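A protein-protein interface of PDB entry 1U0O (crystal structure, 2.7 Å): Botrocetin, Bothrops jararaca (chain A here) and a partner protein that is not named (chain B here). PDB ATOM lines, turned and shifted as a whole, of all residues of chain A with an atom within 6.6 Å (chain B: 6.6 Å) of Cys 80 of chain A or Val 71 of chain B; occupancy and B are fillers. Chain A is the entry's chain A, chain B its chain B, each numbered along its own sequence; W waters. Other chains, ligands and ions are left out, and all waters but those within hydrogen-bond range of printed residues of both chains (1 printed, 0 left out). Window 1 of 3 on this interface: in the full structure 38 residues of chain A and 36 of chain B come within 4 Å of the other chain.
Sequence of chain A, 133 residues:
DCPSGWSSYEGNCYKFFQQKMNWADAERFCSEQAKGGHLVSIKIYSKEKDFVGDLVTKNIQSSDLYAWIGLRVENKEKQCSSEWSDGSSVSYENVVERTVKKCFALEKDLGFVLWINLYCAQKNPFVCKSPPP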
ATOM      1  N   VAL A  73       7.055 -25.532  26.159  1.00  0.00           N
ATOM      2  CA  VAL A  73       8.166 -26.263  26.718  1.00  0.00           C
ATOM      3  C   VAL A  73       7.544 -27.226  27.734  1.00  0.00           C
ATOM      4  O   VAL A  73       6.847 -26.803  28.671  1.00  0.00           O
ATOM      5  CB  VAL A  73       9.119 -25.318  27.440  1.00  0.00           C
ATOM      6  CG1 VAL A  73      10.173 -26.107  28.190  1.00  0.00           C
ATOM      7  CG2 VAL A  73       9.749 -24.381  26.448  1.00  0.00           C
ATOM      8  N   ASN A  75       9.265 -29.084  29.722  1.00  0.00           N
ATOM      9  CA  ASN A  75      10.085 -29.039  30.925  1.00  0.00           C
ATOM     10  C   ASN A  75       9.412 -28.248  32.037  1.00  0.00           C
ATOM     11  O   ASN A  75       8.790 -27.211  31.789  1.00  0.00           O
ATOM     12  CB  ASN A  75      11.434 -28.403  30.634  1.00  0.00           C
ATOM     13  CG  ASN A  75      12.423 -29.374  30.040  1.00  0.00           C
ATOM     14  OD1 ASN A  75      12.201 -29.916  28.958  1.00  0.00           O
ATOM     15  ND2 ASN A  75      13.513 -29.610  30.748  1.00  0.00           N
ATOM     16  N   LYS A  76       9.555 -28.741  33.266  1.00  0.00           N
ATOM     17  CA  LYS A  76       8.965 -28.101  34.439  1.00  0.00           C
ATOM     18  C   LYS A  76       9.969 -27.227  35.186  1.00  0.00           C
ATOM     19  O   LYS A  76       9.569 -26.341  35.940  1.00  0.00           O
ATOM     20  CB  LYS A  76       8.385 -29.151  35.389  1.00  0.00           C
ATOM     21  CG  LYS A  76       7.482 -30.174  34.695  1.00  0.00           C
ATOM     22  CD  LYS A  76       8.147 -31.561  34.623  1.00  0.00           C
ATOM     23  CE  LYS A  76       9.510 -31.536  33.914  1.00  0.00           C
ATOM     24  NZ  LYS A  76      10.168 -32.871  33.938  1.00  0.00           N
ATOM     25  N   GLU A  77      11.265 -27.470  35.004  1.00  0.00           N
ATOM     26  CA  GLU A  77      12.241 -26.611  35.664  1.00  0.00           C
ATOM     27  C   GLU A  77      11.980 -25.245  35.013  1.00  0.00           C
ATOM     28  O   GLU A  77      11.260 -25.166  34.019  1.00  0.00           O
ATOM     29  CB  GLU A  77      13.682 -27.065  35.386  1.00  0.00           C
ATOM     30  CG  GLU A  77      13.994 -28.527  35.714  1.00  0.00           C
ATOM     31  CD  GLU A  77      13.527 -29.492  34.617  1.00  0.00           C
ATOM     32  OE1 GLU A  77      13.959 -29.334  33.445  1.00  0.00           O
ATOM     33  OE2 GLU A  77      12.734 -30.414  34.933  1.00  0.00           O
ATOM     34  N   LYS A  78      12.549 -24.172  35.551  1.00  0.00           N
ATOM     35  CA  LYS A  78      12.294 -22.860  34.967  1.00  0.00           C
ATOM     36  C   LYS A  78      13.076 -22.575  33.685  1.00  0.00           C
ATOM     37  O   LYS A  78      12.736 -21.662  32.933  1.00  0.00           O
ATOM     38  CB  LYS A  78      12.528 -21.753  36.011  1.00  0.00           C
ATOM     39  CG  LYS A  78      11.349 -21.570  36.978  1.00  0.00           C
ATOM     40  CD  LYS A  78      11.601 -20.477  38.006  1.00  0.00           C
ATOM     41  CE  LYS A  78      12.725 -20.874  38.973  1.00  0.00           C
ATOM     42  NZ  LYS A  78      13.127 -19.776  39.909  1.00  0.00           N
ATOM     43  N   GLN A  79      14.119 -23.356  33.441  1.00  0.00           N
ATOM     44  CA  GLN A  79      14.930 -23.208  32.240  1.00  0.00           C
ATOM     45  C   GLN A  79      15.425 -24.617  31.901  1.00  0.00           C
ATOM     46  O   GLN A  79      15.358 -25.500  32.749  1.00  0.00           O
ATOM     47  CB  GLN A  79      16.080 -22.216  32.493  1.00  0.00           C
ATOM     48  CG  GLN A  79      17.145 -22.664  33.462  1.00  0.00           C
ATOM     49  CD  GLN A  79      18.185 -23.539  32.799  1.00  0.00           C
ATOM     50  OE1 GLN A  79      18.737 -23.178  31.765  1.00  0.00           O
ATOM     51  NE2 GLN A  79      18.463 -24.694  33.392  1.00  0.00           N
ATOM     52  N   CYS A  80      15.913 -24.849  30.688  1.00  0.00           N
ATOM     53  CA  CYS A  80      16.329 -26.197  30.336  1.00  0.00           C
ATOM     54  C   CYS A  80      17.805 -26.530  30.186  1.00  0.00           C
ATOM     55  O   CYS A  80      18.153 -27.602  29.696  1.00  0.00           O
ATOM     56  CB  CYS A  80      15.597 -26.620  29.074  1.00  0.00           C
ATOM     57  SG  CYS A  80      13.810 -26.326  29.171  1.00  0.00           S
ATOM     58  N   SER A  81      18.684 -25.630  30.599  1.00  0.00           N
ATOM     59  CA  SER A  81      20.116 -25.904  30.498  1.00  0.00           C
ATOM     60  C   SER A  81      20.468 -26.718  31.732  1.00  0.00           C
ATOM     61  O   SER A  81      20.408 -26.198  32.837  1.00  0.00           O
ATOM     62  CB  SER A  81      20.908 -24.592  30.486  1.00  0.00           C
ATOM     63  OG  SER A  81      22.265 -24.806  30.141  1.00  0.00           O
ATOM     64  N   SER A  82      20.827 -27.988  31.554  1.00  0.00           N
ATOM     65  CA  SER A  82      21.161 -28.848  32.690  1.00  0.00           C
ATOM     66  C   SER A  82      22.640 -28.819  33.094  1.00  0.00           C
ATOM     67  O   SER A  82      23.065 -29.554  33.986  1.00  0.00           O
ATOM     68  CB  SER A  82      20.747 -30.296  32.398  1.00  0.00           C
ATOM     69  OG  SER A  82      21.820 -31.038  31.849  1.00  0.00           O
ATOM     70  N   GLU A  83      23.426 -27.978  32.440  1.00  0.00           N
ATOM     71  CA  GLU A  83      24.839 -27.876  32.772  1.00  0.00           C
ATOM     72  C   GLU A  83      25.347 -26.468  32.530  1.00  0.00           C
ATOM     73  O   GLU A  83      24.917 -25.795  31.588  1.00  0.00           O
ATOM     74  CB  GLU A  83      25.678 -28.833  31.921  1.00  0.00           C
ATOM     75  CG  GLU A  83      25.236 -30.274  31.945  1.00  0.00           C
ATOM     76  CD  GLU A  83      26.243 -31.200  31.273  1.00  0.00           C
ATOM     77  OE1 GLU A  83      27.336 -31.409  31.847  1.00  0.00           O
ATOM     78  OE2 GLU A  83      25.945 -31.711  30.168  1.00  0.00           O
ATOM     79  N   LYS A 102       7.974 -20.220  28.070  1.00  0.00           N
ATOM     80  CA  LYS A 102       7.708 -21.577  27.584  1.00  0.00           C
ATOM     81  C   LYS A 102       6.591 -21.676  26.564  1.00  0.00           C
ATOM     82  O   LYS A 102       6.369 -22.746  26.003  1.00  0.00           O
ATOM     83  CB  LYS A 102       7.337 -22.497  28.742  1.00  0.00           C
ATOM     84  CG  LYS A 102       8.456 -22.769  29.697  1.00  0.00           C
ATOM     85  CD  LYS A 102       7.972 -23.602  30.878  1.00  0.00           C
ATOM     86  CE  LYS A 102       9.065 -23.761  31.912  1.00  0.00           C
ATOM     87  NZ  LYS A 102       8.681 -24.716  32.967  1.00  0.00           N
ATOM     88  N   LEU B  68      25.462 -20.019  31.753  1.00  0.00           N
ATOM     89  CA  LEU B  68      24.326 -20.769  31.214  1.00  0.00           C
ATOM     90  C   LEU B  68      23.847 -20.152  29.908  1.00  0.00           C
ATOM     91  O   LEU B  68      23.607 -18.947  29.848  1.00  0.00           O
ATOM     92  CB  LEU B  68      23.174 -20.780  32.222  1.00  0.00           C
ATOM     93  CG  LEU B  68      23.446 -21.448  33.568  1.00  0.00           C
ATOM     94  CD1 LEU B  68      22.365 -21.057  34.566  1.00  0.00           C
ATOM     95  CD2 LEU B  68      23.527 -22.950  33.371  1.00  0.00           C
ATOM     96  N   SER B  69      23.711 -20.969  28.864  1.00  0.00           N
ATOM     97  CA  SER B  69      23.253 -20.468  27.571  1.00  0.00           C
ATOM     98  C   SER B  69      22.191 -21.336  26.906  1.00  0.00           C
ATOM     99  O   SER B  69      22.010 -22.499  27.267  1.00  0.00           O
ATOM    100  CB  SER B  69      24.417 -20.319  26.603  1.00  0.00           C
ATOM    101  OG  SER B  69      24.939 -21.587  26.279  1.00  0.00           O
ATOM    102  N   ASP B  70      21.518 -20.739  25.916  1.00  0.00           N
ATOM    103  CA  ASP B  70      20.467 -21.373  25.133  1.00  0.00           C
ATOM    104  C   ASP B  70      19.609 -22.312  25.966  1.00  0.00           C
ATOM    105  O   ASP B  70      19.589 -23.523  25.747  1.00  0.00           O
ATOM    106  CB  ASP B  70      21.091 -22.125  23.970  1.00  0.00           C
ATOM    107  CG  ASP B  70      20.102 -22.410  22.878  1.00  0.00           C
ATOM    108  OD1 ASP B  70      19.242 -21.547  22.635  1.00  0.00           O
ATOM    109  OD2 ASP B  70      20.195 -23.480  22.255  1.00  0.00           O
ATOM    110  N   VAL B  71      18.877 -21.729  26.905  1.00  0.00           N
ATOM    111  CA  VAL B  71      18.039 -22.477  27.819  1.00  0.00           C
ATOM    112  C   VAL B  71      16.663 -22.902  27.283  1.00  0.00           C
ATOM    113  O   VAL B  71      15.933 -23.632  27.952  1.00  0.00           O
ATOM    114  CB  VAL B  71      17.842 -21.665  29.122  1.00  0.00           C
ATOM    115  CG1 VAL B  71      19.198 -21.334  29.740  1.00  0.00           C
ATOM    116  CG2 VAL B  71      17.074 -20.385  28.831  1.00  0.00           C
ATOM    117  N   TRP B  72      16.306 -22.466  26.079  1.00  0.00           N
ATOM    118  CA  TRP B  72      15.008 -22.822  25.527  1.00  0.00           C
ATOM    119  C   TRP B  72      15.092 -23.870  24.454  1.00  0.00           C
ATOM    120  O   TRP B  72      14.114 -24.562  24.182  1.00  0.00           O
ATOM    121  CB  TRP B  72      14.329 -21.592  24.958  1.00  0.00           C
ATOM    122  CG  TRP B  72      14.111 -20.575  25.975  1.00  0.00           C
ATOM    123  CD1 TRP B  72      14.380 -19.253  25.878  1.00  0.00           C
ATOM    124  CD2 TRP B  72      13.543 -20.781  27.263  1.00  0.00           C
ATOM    125  NE1 TRP B  72      14.016 -18.609  27.026  1.00  0.00           N
ATOM    126  CE2 TRP B  72      13.493 -19.527  27.897  1.00  0.00           C
ATOM    127  CE3 TRP B  72      13.064 -21.904  27.943  1.00  0.00           C
ATOM    128  CZ2 TRP B  72      12.980 -19.360  29.179  1.00  0.00           C
ATOM    129  CZ3 TRP B  72      12.555 -21.734  29.219  1.00  0.00           C
ATOM    130  CH2 TRP B  72      12.517 -20.468  29.822  1.00  0.00           C
ATOM    131  N   ASN B  73      16.264 -23.992  23.845  1.00  0.00           N
ATOM    132  CA  ASN B  73      16.441 -24.961  22.772  1.00  0.00           C
ATOM    133  C   ASN B  73      16.993 -26.267  23.305  1.00  0.00           C
ATOM    134  O   ASN B  73      17.274 -27.206  22.545  1.00  0.00           O
ATOM    135  CB  ASN B  73      17.340 -24.379  21.675  1.00  0.00           C
ATOM    136  CG  ASN B  73      16.667 -23.260  20.920  1.00  0.00           C
ATOM    137  OD1 ASN B  73      15.553 -23.426  20.417  1.00  0.00           O
ATOM    138  ND2 ASN B  73      17.331 -22.115  20.827  1.00  0.00           N
ATOM    139  N   LYS B  74      17.138 -26.327  24.624  1.00  0.00           N
ATOM    140  CA  LYS B  74      17.622 -27.536  25.260  1.00  0.00           C
ATOM    141  C   LYS B  74      16.398 -28.288  25.810  1.00  0.00           C
ATOM    142  O   LYS B  74      16.450 -29.487  26.123  1.00  0.00           O
ATOM    143  CB  LYS B  74      18.616 -27.170  26.358  1.00  0.00           C
ATOM    144  CG  LYS B  74      19.834 -26.451  25.803  1.00  0.00           C
ATOM    145  CD  LYS B  74      20.867 -26.139  26.866  1.00  0.00           C
ATOM    146  CE  LYS B  74      22.096 -25.549  26.222  1.00  0.00           C
ATOM    147  NZ  LYS B  74      23.127 -25.090  27.210  1.00  0.00           N
ATOM    148  N   CYS B  75      15.288 -27.563  25.878  1.00  0.00           N
ATOM    149  CA  CYS B  75      14.018 -28.097  26.362  1.00  0.00           C
ATOM    150  C   CYS B  75      13.471 -29.192  25.482  1.00  0.00           C
ATOM    151  O   CYS B  75      13.986 -29.462  24.400  1.00  0.00           O
ATOM    152  CB  CYS B  75      12.963 -27.005  26.390  1.00  0.00           C
ATOM    153  SG  CYS B  75      13.397 -25.541  27.358  1.00  0.00           S
ATOM    154  N   ARG B  76      12.404 -29.812  25.956  1.00  0.00           N
ATOM    155  CA  ARG B  76      11.723 -30.839  25.198  1.00  0.00           C
ATOM    156  C   ARG B  76      10.332 -30.240  25.058  1.00  0.00           C
ATOM    157  O   ARG B  76       9.751 -29.812  26.042  1.00  0.00           O
ATOM    158  CB  ARG B  76      11.700 -32.155  25.972  1.00  0.00           C
ATOM    159  CG  ARG B  76      10.752 -32.208  27.137  1.00  0.00           C
ATOM    160  CD  ARG B  76      10.859 -33.557  27.829  1.00  0.00           C
ATOM    161  NE  ARG B  76      11.939 -33.555  28.800  1.00  0.00           N
ATOM    162  CZ  ARG B  76      11.840 -33.032  30.018  1.00  0.00           C
ATOM    163  NH1 ARG B  76      10.703 -32.472  30.420  1.00  0.00           N
ATOM    164  NH2 ARG B  76      12.890 -33.055  30.834  1.00  0.00           N
ATOM    165  N   ALA B  94      13.073 -21.948  19.519  1.00  0.00           N
ATOM    166  CA  ALA B  94      12.958 -20.959  20.595  1.00  0.00           C
ATOM    167  C   ALA B  94      13.955 -19.821  20.437  1.00  0.00           C
ATOM    168  O   ALA B  94      14.737 -19.792  19.491  1.00  0.00           O
ATOM    169  CB  ALA B  94      13.181 -21.634  21.933  1.00  0.00           C
ATOM    170  N   GLU B  95      13.925 -18.874  21.359  1.00  0.00           N
ATOM    171  CA  GLU B  95      14.879 -17.777  21.302  1.00  0.00           C
ATOM    172  C   GLU B  95      16.208 -18.267  21.852  1.00  0.00           C
ATOM    173  O   GLU B  95      16.263 -19.258  22.579  1.00  0.00           O
ATOM    174  CB  GLU B  95      14.403 -16.587  22.136  1.00  0.00           C
ATOM    175  CG  GLU B  95      13.643 -15.572  21.345  1.00  0.00           C
ATOM    176  CD  GLU B  95      14.525 -14.473  20.825  1.00  0.00           C
ATOM    177  OE1 GLU B  95      14.856 -13.577  21.623  1.00  0.00           O
ATOM    178  OE2 GLU B  95      14.894 -14.501  19.631  1.00  0.00           O
ATOM    179  N   TYR B  96      17.279 -17.571  21.501  1.00  0.00           N
ATOM    180  CA  TYR B  96      18.596 -17.931  21.984  1.00  0.00           C
ATOM    181  C   TYR B  96      18.871 -16.996  23.173  1.00  0.00           C
ATOM    182  O   TYR B  96      19.482 -15.933  23.052  1.00  0.00           O
ATOM    183  CB  TYR B  96      19.625 -17.784  20.848  1.00  0.00           C
ATOM    184  CG  TYR B  96      21.025 -18.248  21.190  1.00  0.00           C
ATOM    185  CD1 TYR B  96      22.007 -17.336  21.546  1.00  0.00           C
ATOM    186  CD2 TYR B  96      21.359 -19.599  21.179  1.00  0.00           C
ATOM    187  CE1 TYR B  96      23.285 -17.747  21.885  1.00  0.00           C
ATOM    188  CE2 TYR B  96      22.647 -20.027  21.518  1.00  0.00           C
ATOM    189  CZ  TYR B  96      23.604 -19.089  21.873  1.00  0.00           C
ATOM    190  OH  TYR B  96      24.881 -19.475  22.228  1.00  0.00           O
ATOM    191  N   GLU B  97      18.365 -17.400  24.329  1.00  0.00           N
ATOM    192  CA  GLU B  97      18.534 -16.642  25.559  1.00  0.00           C
ATOM    193  C   GLU B  97      19.511 -17.304  26.533  1.00  0.00           C
ATOM    194  O   GLU B  97      19.675 -18.511  26.544  1.00  0.00           O
ATOM    195  CB  GLU B  97      17.183 -16.451  26.224  1.00  0.00           C
ATOM    196  CG  GLU B  97      16.174 -15.843  25.302  1.00  0.00           C
ATOM    197  CD  GLU B  97      15.156 -15.057  26.057  1.00  0.00           C
ATOM    198  OE1 GLU B  97      14.539 -15.632  26.981  1.00  0.00           O
ATOM    199  OE2 GLU B  97      14.982 -13.862  25.721  1.00  0.00           O
ATOM    200  N   CYS B  98      20.156 -16.487  27.346  1.00  0.00           N
ATOM    201  CA  CYS B  98      21.154 -16.958  28.298  1.00  0.00           C
ATOM    202  C   CYS B  98      20.829 -16.344  29.665  1.00  0.00           C
ATOM    203  O   CYS B  98      19.938 -15.496  29.762  1.00  0.00           O
ATOM    204  CB  CYS B  98      22.548 -16.538  27.804  1.00  0.00           C
ATOM    205  SG  CYS B  98      23.126 -17.313  26.230  1.00  0.00           S
ATOM    206  N   VAL B  99      21.545 -16.757  30.711  1.00  0.00           N
ATOM    207  CA  VAL B  99      21.276 -16.266  32.063  1.00  0.00           C
ATOM    208  C   VAL B  99      22.179 -15.166  32.600  1.00  0.00           C
ATOM    209  O   VAL B  99      23.403 -15.259  32.510  1.00  0.00           O
ATOM    210  CB  VAL B  99      21.341 -17.413  33.077  1.00  0.00           C
ATOM    211  CG1 VAL B  99      20.849 -16.939  34.427  1.00  0.00           C
ATOM    212  CG2 VAL B  99      20.521 -18.572  32.587  1.00  0.00           C
ATOM    213  N   ILE B 110      16.727 -14.490  32.526  1.00  0.00           N
ATOM    214  CA  ILE B 110      16.912 -15.237  31.288  1.00  0.00           C
ATOM    215  C   ILE B 110      16.640 -14.215  30.189  1.00  0.00           C
ATOM    216  O   ILE B 110      15.481 -13.837  29.939  1.00  0.00           O
ATOM    217  CB  ILE B 110      15.916 -16.407  31.152  1.00  0.00           C
ATOM    218  CG1 ILE B 110      16.081 -17.371  32.339  1.00  0.00           C
ATOM    219  CG2 ILE B 110      16.118 -17.088  29.792  1.00  0.00           C
ATOM    220  CD1 ILE B 110      14.994 -18.435  32.455  1.00  0.00           C
ATOM    221  N   ILE B 111      17.704 -13.750  29.542  1.00  0.00           N
ATOM    222  CA  ILE B 111      17.550 -12.746  28.501  1.00  0.00           C
ATOM    223  C   ILE B 111      18.187 -13.203  27.201  1.00  0.00           C
ATOM    224  O   ILE B 111      18.781 -14.271  27.146  1.00  0.00           O
ATOM    225  CB  ILE B 111      18.164 -11.378  28.952  1.00  0.00           C
ATOM    226  CG1 ILE B 111      19.562 -11.594  29.523  1.00  0.00           C
ATOM    227  CG2 ILE B 111      17.233 -10.699  29.975  1.00  0.00           C
ATOM    228  CD1 ILE B 111      19.700 -12.263  30.878  1.00  0.00           C
ATOM    229  N   CYS B 113      20.839 -13.703  24.389  1.00  0.00           N
ATOM    230  CA  CYS B 113      22.300 -13.751  24.470  1.00  0.00           C
ATOM    231  C   CYS B 113      23.025 -12.665  23.659  1.00  0.00           C
ATOM    232  O   CYS B 113      24.241 -12.530  23.753  1.00  0.00           O
ATOM    233  CB  CYS B 113      22.814 -15.128  24.031  1.00  0.00           C
ATOM    234  SG  CYS B 113      21.947 -16.558  24.752  1.00  0.00           S
HETATM  235  O   HOH W   1      24.816 -24.089  29.462  1.00  0.00           O
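The side-chain amide oxygen (OD1) of Asn 75 of chain A is in hydrogen-bond range of the backbone NH (N) of Arg 76 of chain B, at 3.0 Å.
The backbone NH (N) of Cys 80 of chain A sits at hydrogen-bond distance from the backbone carbonyl oxygen (O) of Val 71 of chain B (3.0 Å).
The side-chain sulfur (SG) of Cys 80 of chain A is disulfide-bonded to the side-chain sulfur (SG) of Cys 75 of chain B (2.0 Å).
NZ of Lys 74 of chain B lies within hydrogen-bond range of OG of Ser 81 of chain A (3.1 Å).
Water W1 lies within hydrogen-bond range of O of Glu 83 of chain A (2.7 Å), OG of Ser 81 of chain A (2.7 Å), NZ of Lys 74 of chain B (3.0 Å) and N of Ser 69 of chain B (3.4 Å).
CG1 of Val 73 of chain A touches SG of Cys 75 of chain B, at 3.4 Å.
C of Val 73 of chain A touches O of Arg 76 of chain B, at 3.8 Å.
Trp 72 of chain B touches Lys 78 of chain A.
Ile 110 of chain B touches Lys 78 of chain A.
Gln 79 of chain A touches Val 71 of chain B (OE1 to CG1, 2.8 Å).
CD1 of Ile 110 of chain B touches CB of Gln 79 of chain A, at 3.9 Å.
Lys 74 of chain B touches Cys 80 of chain A (CB to O, 3.4 Å).
O of Ser 69 of chain B touches OG of Ser 81 of chain A (3.7 Å).
CB of Ser 81 of chain A touches CG1 of Val 71 of chain B (3.8 Å).
CD2 of Leu 68 of chain B touches O of Glu 83 of chain A, at 3.6 Å.
Of the 18 printed residues of chain B, 8 touch a printed residue of chain A.
Hydrophobic or aromatic side chains of chain B that line the printed part of chain A: Leu 68, Val 71, Trp 72 and Ile 110.
Hydrophobic or aromatic side chains of chain A that line the printed part of chain B: Val 73.
Among the printed residues, 17 pairs touch across the chains.
Among the printed residues, no Asp or Glu carboxylate lies within 4 Å of a Lys or Arg side-chain nitrogen of the other chain.
Of chain B, only Val 71, Lys 74 and Cys 75 come within 4 Å of Cys 80 of chain A.
Val 71 of chain B touches just these residues of chain A: Gln 79, Cys 80 and Ser 81.
Of the printed residues of chain B, Lys 78 of chain A touches Trp 72 and Ile 110.
Of the printed residues of chain B, Lys 76 of chain A touches Arg 76.
Printed residues of chain A within 4 Å of Ile 110 of chain B: Lys 78 and Gln 79.
Cys 98 of chain B touches none of the printed residues of chain A.
The nearest residue of chain B that does not touch Cys 80 of chain A is Trp 72 of chain B (4.6 Å).
The nearest printed residue of chain A that does not touch Ser 69 of chain B is Gln 79 of chain A (5.6 Å).
The backbone NH (N) of Val 73 of chain A is in hydrogen-bond range of the backbone carbonyl oxygen (O) of Lys 102 of chain A (2.9 Å).
OE1 of Glu 77 of chain A lies within hydrogen-bond range of ND2 of Asn 75 of chain A.
The backbone carbonyl oxygen (O) of Asn 75 of chain A sits at hydrogen-bond distance from the side-chain amino group (NZ) of Lys 102 of chain A (2.8 Å).
The side-chain carboxylate (OE2) of Glu 77 of chain A is in salt-bridge range of the side-chain amino group (NZ) of Lys 76 of chain A, at 3.7 Å.
The side-chain hydroxyl (OG) of Ser 81 of chain A is in hydrogen-bond range of the backbone carbonyl oxygen (O) of Glu 83 of chain A (3.2 Å).
The backbone carbonyl oxygen (O) of Leu 68 of chain B is in hydrogen-bond range of the backbone NH (N) of Val 99 of chain B (3.1 Å).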
